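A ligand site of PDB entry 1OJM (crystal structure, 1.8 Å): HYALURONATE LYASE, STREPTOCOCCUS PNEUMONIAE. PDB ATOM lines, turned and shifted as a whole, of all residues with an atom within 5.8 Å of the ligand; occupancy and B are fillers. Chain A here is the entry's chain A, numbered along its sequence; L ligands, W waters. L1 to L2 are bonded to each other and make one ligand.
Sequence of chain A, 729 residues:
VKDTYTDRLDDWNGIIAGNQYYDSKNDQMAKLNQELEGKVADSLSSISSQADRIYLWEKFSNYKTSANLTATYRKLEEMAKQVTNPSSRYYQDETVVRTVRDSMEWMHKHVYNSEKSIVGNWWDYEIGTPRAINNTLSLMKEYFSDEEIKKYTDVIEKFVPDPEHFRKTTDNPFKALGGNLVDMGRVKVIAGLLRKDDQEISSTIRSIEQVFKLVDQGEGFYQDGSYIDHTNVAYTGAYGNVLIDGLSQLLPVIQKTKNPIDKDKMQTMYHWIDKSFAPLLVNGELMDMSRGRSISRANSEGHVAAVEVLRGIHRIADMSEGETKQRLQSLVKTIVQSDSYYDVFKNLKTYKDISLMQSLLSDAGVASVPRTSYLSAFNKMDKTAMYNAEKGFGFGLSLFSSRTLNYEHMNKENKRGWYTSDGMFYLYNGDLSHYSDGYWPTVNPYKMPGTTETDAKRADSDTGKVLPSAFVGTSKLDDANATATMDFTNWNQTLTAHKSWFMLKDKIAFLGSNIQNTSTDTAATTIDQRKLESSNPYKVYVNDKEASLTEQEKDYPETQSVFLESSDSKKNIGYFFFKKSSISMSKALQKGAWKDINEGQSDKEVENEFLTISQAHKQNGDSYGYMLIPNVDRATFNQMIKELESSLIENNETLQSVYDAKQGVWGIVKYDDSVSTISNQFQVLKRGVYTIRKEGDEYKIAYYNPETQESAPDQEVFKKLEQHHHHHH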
ATOM      1  N   ARG A  74      -6.158   9.138 -32.913  1.00  0.00           N
ATOM      2  CA  ARG A  74      -7.271   8.754 -33.772  1.00  0.00           C
ATOM      3  C   ARG A  74      -7.191   9.466 -35.127  1.00  0.00           C
ATOM      4  O   ARG A  74      -7.663   8.938 -36.126  1.00  0.00           O
ATOM      5  CB  ARG A  74      -8.610   9.027 -33.072  1.00  0.00           C
ATOM      6  CG  ARG A  74      -8.950   7.925 -32.075  1.00  0.00           C
ATOM      7  CD  ARG A  74     -10.288   8.123 -31.386  1.00  0.00           C
ATOM      8  NE  ARG A  74     -10.599   6.959 -30.561  1.00  0.00           N
ATOM      9  CZ  ARG A  74     -11.707   6.802 -29.849  1.00  0.00           C
ATOM     10  NH1 ARG A  74     -11.882   5.701 -29.132  1.00  0.00           N
ATOM     11  NH2 ARG A  74     -12.634   7.748 -29.844  1.00  0.00           N
ATOM     12  N   ASN A 121      -7.538  11.127 -17.393  1.00  0.00           N
ATOM     13  CA  ASN A 121      -8.336   9.897 -17.339  1.00  0.00           C
ATOM     14  C   ASN A 121      -7.563   8.650 -17.749  1.00  0.00           C
ATOM     15  O   ASN A 121      -6.940   8.609 -18.816  1.00  0.00           O
ATOM     16  CB  ASN A 121      -9.571  10.056 -18.229  1.00  0.00           C
ATOM     17  CG  ASN A 121     -10.688   9.108 -17.832  1.00  0.00           C
ATOM     18  OD1 ASN A 121     -10.529   7.892 -17.858  1.00  0.00           O
ATOM     19  ND2 ASN A 121     -11.833   9.676 -17.453  1.00  0.00           N
ATOM     20  N   TRP A 123      -8.643   5.891 -18.841  1.00  0.00           N
ATOM     21  CA  TRP A 123      -9.191   5.295 -20.066  1.00  0.00           C
ATOM     22  C   TRP A 123      -8.388   5.647 -21.319  1.00  0.00           C
ATOM     23  O   TRP A 123      -8.137   4.788 -22.175  1.00  0.00           O
ATOM     24  CB  TRP A 123     -10.643   5.728 -20.244  1.00  0.00           C
ATOM     25  CG  TRP A 123     -11.353   4.978 -21.327  1.00  0.00           C
ATOM     26  CD1 TRP A 123     -12.020   3.784 -21.207  1.00  0.00           C
ATOM     27  CD2 TRP A 123     -11.466   5.347 -22.711  1.00  0.00           C
ATOM     28  NE1 TRP A 123     -12.545   3.405 -22.416  1.00  0.00           N
ATOM     29  CE2 TRP A 123     -12.225   4.343 -23.357  1.00  0.00           C
ATOM     30  CE3 TRP A 123     -11.001   6.443 -23.450  1.00  0.00           C
ATOM     31  CZ2 TRP A 123     -12.518   4.396 -24.723  1.00  0.00           C
ATOM     32  CZ3 TRP A 123     -11.303   6.502 -24.812  1.00  0.00           C
ATOM     33  CH2 TRP A 123     -12.057   5.483 -25.434  1.00  0.00           C
ATOM     34  N   ASP A 124      -8.022   6.917 -21.448  1.00  0.00           N
ATOM     35  CA  ASP A 124      -7.260   7.373 -22.603  1.00  0.00           C
ATOM     36  C   ASP A 124      -5.900   6.673 -22.671  1.00  0.00           C
ATOM     37  O   ASP A 124      -5.478   6.235 -23.738  1.00  0.00           O
ATOM     38  CB  ASP A 124      -7.073   8.879 -22.560  1.00  0.00           C
ATOM     39  CG  ASP A 124      -8.351   9.634 -22.802  1.00  0.00           C
ATOM     40  OD1 ASP A 124      -8.969   9.438 -23.884  1.00  0.00           O
ATOM     41  OD2 ASP A 124      -8.754  10.433 -21.925  1.00  0.00           O
ATOM     42  N   ARG A 131      -5.698   1.511 -28.427  1.00  0.00           N
ATOM     43  CA  ARG A 131      -6.508   1.041 -29.539  1.00  0.00           C
ATOM     44  C   ARG A 131      -6.191   1.803 -30.836  1.00  0.00           C
ATOM     45  O   ARG A 131      -6.091   1.202 -31.898  1.00  0.00           O
ATOM     46  CB  ARG A 131      -8.003   1.176 -29.216  1.00  0.00           C
ATOM     47  CG  ARG A 131      -8.573   0.035 -28.380  1.00  0.00           C
ATOM     48  CD  ARG A 131      -9.989   0.366 -27.906  1.00  0.00           C
ATOM     49  NE  ARG A 131     -10.819   0.816 -29.019  1.00  0.00           N
ATOM     50  CZ  ARG A 131     -11.943   1.514 -28.881  1.00  0.00           C
ATOM     51  NH1 ARG A 131     -12.379   1.848 -27.666  1.00  0.00           N
ATOM     52  NH2 ARG A 131     -12.625   1.901 -29.953  1.00  0.00           N
ATOM     53  N   ASN A 180     -15.385  -3.089 -20.776  1.00  0.00           N
ATOM     54  CA  ASN A 180     -13.975  -2.820 -20.506  1.00  0.00           C
ATOM     55  C   ASN A 180     -13.130  -4.036 -20.835  1.00  0.00           C
ATOM     56  O   ASN A 180     -12.060  -3.909 -21.436  1.00  0.00           O
ATOM     57  CB  ASN A 180     -13.777  -2.445 -19.034  1.00  0.00           C
ATOM     58  CG  ASN A 180     -14.264  -1.039 -18.724  1.00  0.00           C
ATOM     59  OD1 ASN A 180     -14.596  -0.735 -17.568  1.00  0.00           O
ATOM     60  ND2 ASN A 180     -14.295  -0.176 -19.720  1.00  0.00           N
ATOM     61  N   ARG A 186      -9.161  -5.650 -27.415  1.00  0.00           N
ATOM     62  CA  ARG A 186      -8.784  -4.803 -28.539  1.00  0.00           C
ATOM     63  C   ARG A 186      -7.466  -4.065 -28.281  1.00  0.00           C
ATOM     64  O   ARG A 186      -6.881  -3.493 -29.193  1.00  0.00           O
ATOM     65  CB  ARG A 186      -9.900  -3.797 -28.859  1.00  0.00           C
ATOM     66  CG  ARG A 186     -11.175  -4.502 -29.376  1.00  0.00           C
ATOM     67  CD  ARG A 186     -12.148  -3.561 -30.093  1.00  0.00           C
ATOM     68  NE  ARG A 186     -12.758  -2.572 -29.197  1.00  0.00           N
ATOM     69  CZ  ARG A 186     -13.722  -1.737 -29.565  1.00  0.00           C
ATOM     70  NH1 ARG A 186     -14.179  -1.756 -30.816  1.00  0.00           N
ATOM     71  NH2 ARG A 186     -14.211  -0.863 -28.697  1.00  0.00           N
ATOM     72  N   HIS A 230     -20.480  -0.379 -13.754  1.00  0.00           N
ATOM     73  CA  HIS A 230     -20.189   0.648 -12.776  1.00  0.00           C
ATOM     74  C   HIS A 230     -20.869   0.337 -11.452  1.00  0.00           C
ATOM     75  O   HIS A 230     -21.571   1.173 -10.862  1.00  0.00           O
ATOM     76  CB  HIS A 230     -20.613   2.028 -13.299  1.00  0.00           C
ATOM     77  CG  HIS A 230     -19.682   2.570 -14.346  1.00  0.00           C
ATOM     78  ND1 HIS A 230     -19.852   3.806 -14.925  1.00  0.00           N
ATOM     79  CD2 HIS A 230     -18.576   2.030 -14.910  1.00  0.00           C
ATOM     80  CE1 HIS A 230     -18.883   4.015 -15.800  1.00  0.00           C
ATOM     81  NE2 HIS A 230     -18.096   2.961 -15.804  1.00  0.00           N
ATOM     82  N   TYR A 235     -26.922  -0.754 -17.584  1.00  0.00           N
ATOM     83  CA  TYR A 235     -26.098  -0.218 -18.660  1.00  0.00           C
ATOM     84  C   TYR A 235     -25.994  -0.978 -19.980  1.00  0.00           C
ATOM     85  O   TYR A 235     -25.019  -0.806 -20.721  1.00  0.00           O
ATOM     86  CB  TYR A 235     -24.675   0.014 -18.117  1.00  0.00           C
ATOM     87  CG  TYR A 235     -24.252   1.458 -18.113  1.00  0.00           C
ATOM     88  CD1 TYR A 235     -24.486   2.269 -19.224  1.00  0.00           C
ATOM     89  CD2 TYR A 235     -23.600   2.017 -17.017  1.00  0.00           C
ATOM     90  CE1 TYR A 235     -24.090   3.600 -19.240  1.00  0.00           C
ATOM     91  CE2 TYR A 235     -23.191   3.360 -17.020  1.00  0.00           C
ATOM     92  CZ  TYR A 235     -23.437   4.136 -18.140  1.00  0.00           C
ATOM     93  OH  TYR A 235     -23.063   5.445 -18.174  1.00  0.00           O
ATOM     94  N   ALA A 238     -24.942   1.051 -23.383  1.00  0.00           N
ATOM     95  CA  ALA A 238     -23.733   1.849 -23.593  1.00  0.00           C
ATOM     96  C   ALA A 238     -22.532   0.934 -23.415  1.00  0.00           C
ATOM     97  O   ALA A 238     -21.791   0.692 -24.360  1.00  0.00           O
ATOM     98  CB  ALA A 238     -23.681   3.018 -22.604  1.00  0.00           C
ATOM     99  N   TYR A 239     -22.341   0.399 -22.213  1.00  0.00           N
ATOM    100  CA  TYR A 239     -21.235  -0.512 -21.977  1.00  0.00           C
ATOM    101  C   TYR A 239     -21.510  -1.859 -22.640  1.00  0.00           C
ATOM    102  O   TYR A 239     -20.591  -2.518 -23.135  1.00  0.00           O
ATOM    103  CB  TYR A 239     -20.970  -0.645 -20.472  1.00  0.00           C
ATOM    104  CG  TYR A 239     -20.202   0.544 -19.951  1.00  0.00           C
ATOM    105  CD1 TYR A 239     -18.840   0.685 -20.210  1.00  0.00           C
ATOM    106  CD2 TYR A 239     -20.856   1.589 -19.289  1.00  0.00           C
ATOM    107  CE1 TYR A 239     -18.134   1.825 -19.832  1.00  0.00           C
ATOM    108  CE2 TYR A 239     -20.168   2.746 -18.915  1.00  0.00           C
ATOM    109  CZ  TYR A 239     -18.821   2.859 -19.196  1.00  0.00           C
ATOM    110  OH  TYR A 239     -18.152   4.024 -18.872  1.00  0.00           O
ATOM    111  N   VAL A 242     -20.574  -1.443 -26.273  1.00  0.00           N
ATOM    112  CA  VAL A 242     -19.134  -1.561 -26.446  1.00  0.00           C
ATOM    113  C   VAL A 242     -18.729  -3.037 -26.430  1.00  0.00           C
ATOM    114  O   VAL A 242     -17.942  -3.481 -27.268  1.00  0.00           O
ATOM    115  CB  VAL A 242     -18.389  -0.815 -25.313  1.00  0.00           C
ATOM    116  CG1 VAL A 242     -16.907  -1.168 -25.323  1.00  0.00           C
ATOM    117  CG2 VAL A 242     -18.587   0.682 -25.473  1.00  0.00           C
ATOM    118  N   ARG A 293     -25.208   7.600 -18.884  1.00  0.00           N
ATOM    119  CA  ARG A 293     -24.835   8.979 -19.182  1.00  0.00           C
ATOM    120  C   ARG A 293     -24.667   9.290 -20.667  1.00  0.00           C
ATOM    121  O   ARG A 293     -24.593  10.449 -21.047  1.00  0.00           O
ATOM    122  CB  ARG A 293     -23.555   9.354 -18.436  1.00  0.00           C
ATOM    123  CG  ARG A 293     -22.278   8.684 -18.936  1.00  0.00           C
ATOM    124  CD  ARG A 293     -21.082   9.073 -18.070  1.00  0.00           C
ATOM    125  NE  ARG A 293     -19.811   8.836 -18.746  1.00  0.00           N
ATOM    126  CZ  ARG A 293     -19.187   7.660 -18.804  1.00  0.00           C
ATOM    127  NH1 ARG A 293     -19.710   6.591 -18.213  1.00  0.00           N
ATOM    128  NH2 ARG A 293     -18.046   7.552 -19.486  1.00  0.00           N
ATOM    129  N   SER A 294     -24.630   8.253 -21.511  1.00  0.00           N
ATOM    130  CA  SER A 294     -24.477   8.438 -22.951  1.00  0.00           C
ATOM    131  C   SER A 294     -25.645   9.192 -23.606  1.00  0.00           C
ATOM    132  O   SER A 294     -25.514   9.656 -24.742  1.00  0.00           O
ATOM    133  CB  SER A 294     -24.297   7.089 -23.642  1.00  0.00           C
ATOM    134  OG  SER A 294     -22.961   6.662 -23.500  1.00  0.00           O
ATOM    135  N   ARG A 297     -24.942  12.741 -25.032  1.00  0.00           N
ATOM    136  CA  ARG A 297     -24.004  12.928 -26.147  1.00  0.00           C
ATOM    137  C   ARG A 297     -24.800  13.174 -27.431  1.00  0.00           C
ATOM    138  O   ARG A 297     -25.538  12.301 -27.889  1.00  0.00           O
ATOM    139  CB  ARG A 297     -23.120  11.685 -26.316  1.00  0.00           C
ATOM    140  CG  ARG A 297     -22.223  11.421 -25.114  1.00  0.00           C
ATOM    141  CD  ARG A 297     -21.544  10.070 -25.207  1.00  0.00           C
ATOM    142  NE  ARG A 297     -20.839   9.741 -23.981  1.00  0.00           N
ATOM    143  CZ  ARG A 297     -20.393   8.536 -23.674  1.00  0.00           C
ATOM    144  NH1 ARG A 297     -20.580   7.528 -24.517  1.00  0.00           N
ATOM    145  NH2 ARG A 297     -19.756   8.326 -22.525  1.00  0.00           N
ATOM    146  N   SER A 300     -24.815  10.632 -30.257  1.00  0.00           N
ATOM    147  CA  SER A 300     -25.226   9.283 -29.894  1.00  0.00           C
ATOM    148  C   SER A 300     -26.674   9.140 -29.451  1.00  0.00           C
ATOM    149  O   SER A 300     -26.956   8.477 -28.457  1.00  0.00           O
ATOM    150  CB  SER A 300     -24.317   8.763 -28.768  1.00  0.00           C
ATOM    151  OG  SER A 300     -22.953   8.823 -29.156  1.00  0.00           O
ATOM    152  N   GLU A 308     -24.908   0.612 -33.140  1.00  0.00           N
ATOM    153  CA  GLU A 308     -23.728   0.057 -32.496  1.00  0.00           C
ATOM    154  C   GLU A 308     -24.005  -1.396 -32.147  1.00  0.00           C
ATOM    155  O   GLU A 308     -23.156  -2.269 -32.320  1.00  0.00           O
ATOM    156  CB  GLU A 308     -23.403   0.777 -31.182  1.00  0.00           C
ATOM    157  CG  GLU A 308     -22.491   1.964 -31.286  1.00  0.00           C
ATOM    158  CD  GLU A 308     -21.925   2.332 -29.932  1.00  0.00           C
ATOM    159  OE1 GLU A 308     -22.721   2.428 -28.973  1.00  0.00           O
ATOM    160  OE2 GLU A 308     -20.694   2.520 -29.822  1.00  0.00           O
ATOM    161  N   ASN A 411     -17.597  12.081 -15.554  1.00  0.00           N
ATOM    162  CA  ASN A 411     -16.785  12.598 -16.656  1.00  0.00           C
ATOM    163  C   ASN A 411     -17.475  13.820 -17.220  1.00  0.00           C
ATOM    164  O   ASN A 411     -17.383  14.115 -18.407  1.00  0.00           O
ATOM    165  CB  ASN A 411     -16.572  11.543 -17.735  1.00  0.00           C
ATOM    166  CG  ASN A 411     -15.538  10.500 -17.333  1.00  0.00           C
ATOM    167  OD1 ASN A 411     -14.785  10.707 -16.374  1.00  0.00           O
ATOM    168  ND2 ASN A 411     -15.480   9.402 -18.059  1.00  0.00           N
ATOM    169  N   GLU A 413     -20.534  14.276 -17.701  1.00  0.00           N
ATOM    170  CA  GLU A 413     -21.632  13.906 -18.595  1.00  0.00           C
ATOM    171  C   GLU A 413     -22.912  13.585 -17.828  1.00  0.00           C
ATOM    172  O   GLU A 413     -22.872  12.971 -16.755  1.00  0.00           O
ATOM    173  CB  GLU A 413     -21.244  12.699 -19.443  1.00  0.00           C
ATOM    174  CG  GLU A 413     -19.953  12.867 -20.235  1.00  0.00           C
ATOM    175  CD  GLU A 413     -19.721  11.719 -21.188  1.00  0.00           C
ATOM    176  OE1 GLU A 413     -19.346  10.630 -20.705  1.00  0.00           O
ATOM    177  OE2 GLU A 413     -19.934  11.911 -22.405  1.00  0.00           O
HETATM  178  C1  LIG L   1     -15.720   5.564 -21.385  1.00  0.00           C
HETATM  179  C2  LIG L   1     -16.886   5.673 -22.379  1.00  0.00           C
HETATM  180  C3  LIG L   1     -16.319   6.036 -23.764  1.00  0.00           C
HETATM  181  C4  LIG L   1     -15.533   7.395 -23.716  1.00  0.00           C
HETATM  182  C5  LIG L   1     -14.394   7.254 -22.711  1.00  0.00           C
HETATM  183  C6  LIG L   1     -13.624   8.562 -22.609  1.00  0.00           C
HETATM  184  C7  LIG L   1     -19.101   4.445 -22.323  1.00  0.00           C
HETATM  185  C8  LIG L   1     -19.776   3.103 -22.525  1.00  0.00           C
HETATM  186  N1  LIG L   1     -17.683   4.379 -22.528  1.00  0.00           N
HETATM  187  O1  LIG L   1     -16.222   5.239 -20.095  1.00  0.00           O
HETATM  188  O2  LIG L   1     -17.445   6.090 -24.664  1.00  0.00           O
HETATM  189  O3  LIG L   1     -16.474   8.385 -23.462  1.00  0.00           O
HETATM  190  O4  LIG L   1     -14.967   6.859 -21.353  1.00  0.00           O
HETATM  191  O5  LIG L   1     -12.651   8.557 -21.516  1.00  0.00           O
HETATM  192  O6  LIG L   1     -19.734   5.494 -22.031  1.00  0.00           O
HETATM  193  C1  LG2 L   2     -17.563   5.137 -25.691  1.00  0.00           C
HETATM  194  C2  LG2 L   2     -18.822   5.331 -26.466  1.00  0.00           C
HETATM  195  C3  LG2 L   2     -18.827   4.240 -27.606  1.00  0.00           C
HETATM  196  C4  LG2 L   2     -17.500   3.896 -28.320  1.00  0.00           C
HETATM  197  C5  LG2 L   2     -16.358   4.482 -27.876  1.00  0.00           C
HETATM  198  C6  LG2 L   2     -14.990   4.255 -28.471  1.00  0.00           C
HETATM  199  O1  LG2 L   2     -19.970   5.091 -25.581  1.00  0.00           O
HETATM  200  O2  LG2 L   2     -19.983   4.544 -28.383  1.00  0.00           O
HETATM  201  O3  LG2 L   2     -16.426   5.421 -26.673  1.00  0.00           O
HETATM  202  O4  LG2 L   2     -14.872   3.307 -29.334  1.00  0.00           O
HETATM  203  O5  LG2 L   2     -14.128   5.066 -27.994  1.00  0.00           O
HETATM  204  O   HOH W   1     -22.293   5.869 -21.054  1.00  0.00           O
HETATM  205  O   HOH W   2     -12.898  11.941 -23.099  1.00  0.00           O
HETATM  206  O   HOH W   3     -11.178  10.813 -21.269  1.00  0.00           O
HETATM  207  O   HOH W   4     -16.230   0.964 -28.610  1.00  0.00           O
HETATM  208  O   HOH W   5     -16.745   9.791 -21.142  1.00  0.00           O
HETATM  209  O   HOH W   6     -16.048   2.848 -31.651  1.00  0.00           O
HETATM  210  O   HOH W   7     -16.082   2.398 -23.447  1.00  0.00           O
HETATM  211  O   HOH W   8     -21.847   7.237 -27.144  1.00  0.00           O
HETATM  212  O   HOH W   9     -13.342   7.282 -18.852  1.00  0.00           O
HETATM  213  O   HOH W  10     -14.694   2.522 -19.336  1.00  0.00           O
HETATM  214  O   HOH W  11     -14.318   4.967 -18.262  1.00  0.00           O
HETATM  215  O   HOH W  12     -17.666   9.333 -25.772  1.00  0.00           O
HETATM  216  O   HOH W  13     -14.531   7.672 -27.507  1.00  0.00           O
HETATM  217  O   HOH W  14     -21.791   3.005 -26.170  1.00  0.00           O
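An oxygen (O2) of LG2 L2 is in hydrogen-bond range of the side-chain carboxylate of Glu 308 (2.6 Å). O1 of LIG L1 lies within hydrogen-bond range of OH of Tyr 239 (2.6 Å). NH1 of Arg 74 is in salt-bridge range of O5 of LG2 L2, 2.6 Å away. The guanidinium group of Arg 131 lies within salt-bridge range of an oxygen (O4) of LG2 L2 (2.7 Å). NH1 of Arg 297 lies within hydrogen-bond range of O1 of LG2 L2 (2.7 Å). An oxygen (O1) of LIG L1 lies within hydrogen-bond range of the guanidinium group of Arg 293.
Residues that only touch the ligand: Trp 123, Ala 238, Val 242 and Ser 294. Ten residues have an atom within 4 Å of the ligand: Arg 74, Trp 123, Arg 131, Ala 238, Tyr 239, Val 242, Arg 293, Ser 294, Arg 297 and Glu 308. Along chain A the residues within 4 Å of the ligand span positions 74 to 308.
The side-chain hydroxyl (OH) of Tyr 239 sits at hydrogen-bond distance from the guanidinium group (NH1) of Arg 293, 3.1 Å away. OH of Tyr 239 sits close to NE2 of His 230 (3.2 Å). The guanidinium group (NH1) of Arg 297 sits at hydrogen-bond distance from the side-chain hydroxyl (OG) of Ser 294, 2.7 Å away. The guanidinium group (NE) of Arg 297 lies within salt-bridge range of the side-chain carboxylate (OE2) of Glu 413 (2.8 Å). The side-chain amide nitrogen (ND2) of Asn 411 lies close to the guanidinium group (NH2) of Arg 293 (3.5 Å). NE of Arg 293 is in salt-bridge range of OE1 of Glu 413. The backbone NH of Arg 293 sits at hydrogen-bond distance from the side-chain hydroxyl of Tyr 235, 3.1 Å away. The side-chain amide oxygen (OD1) of Asn 121 sits at hydrogen-bond distance from the backbone NH (N) of Trp 123, 2.9 Å away.
Water W13 bridges O5 of LG2 L2 and NH2 of Arg 74. Water W5 lies within hydrogen-bond range of an oxygen (O3) of LIG L1 (2.7 Å), the side-chain carboxylate of Glu 413 (2.8 Å), the guanidinium group of Arg 293 (3.1 Å) and the side-chain amide nitrogen of Asn 411 (3.4 Å). Water W1 lies within hydrogen-bond range of OG of Ser 294 (2.7 Å), O6 of LIG L1 (2.8 Å) and OH of Tyr 235 (3.0 Å). Water W4 lies within hydrogen-bond range of the guanidinium group (NH2) of Arg 186 and an oxygen (O4) of LG2 L2. Water W14 lies within hydrogen-bond range of O1 of LG2 L2, O of Ala 238 and OE1 of Glu 308. Water W9 lies within hydrogen-bond range of an oxygen (O4) of LIG L1 (3.0 Å), the side-chain amide oxygen of Asn 121 (3.0 Å) and the side-chain amide nitrogen of Asn 411 (3.1 Å).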
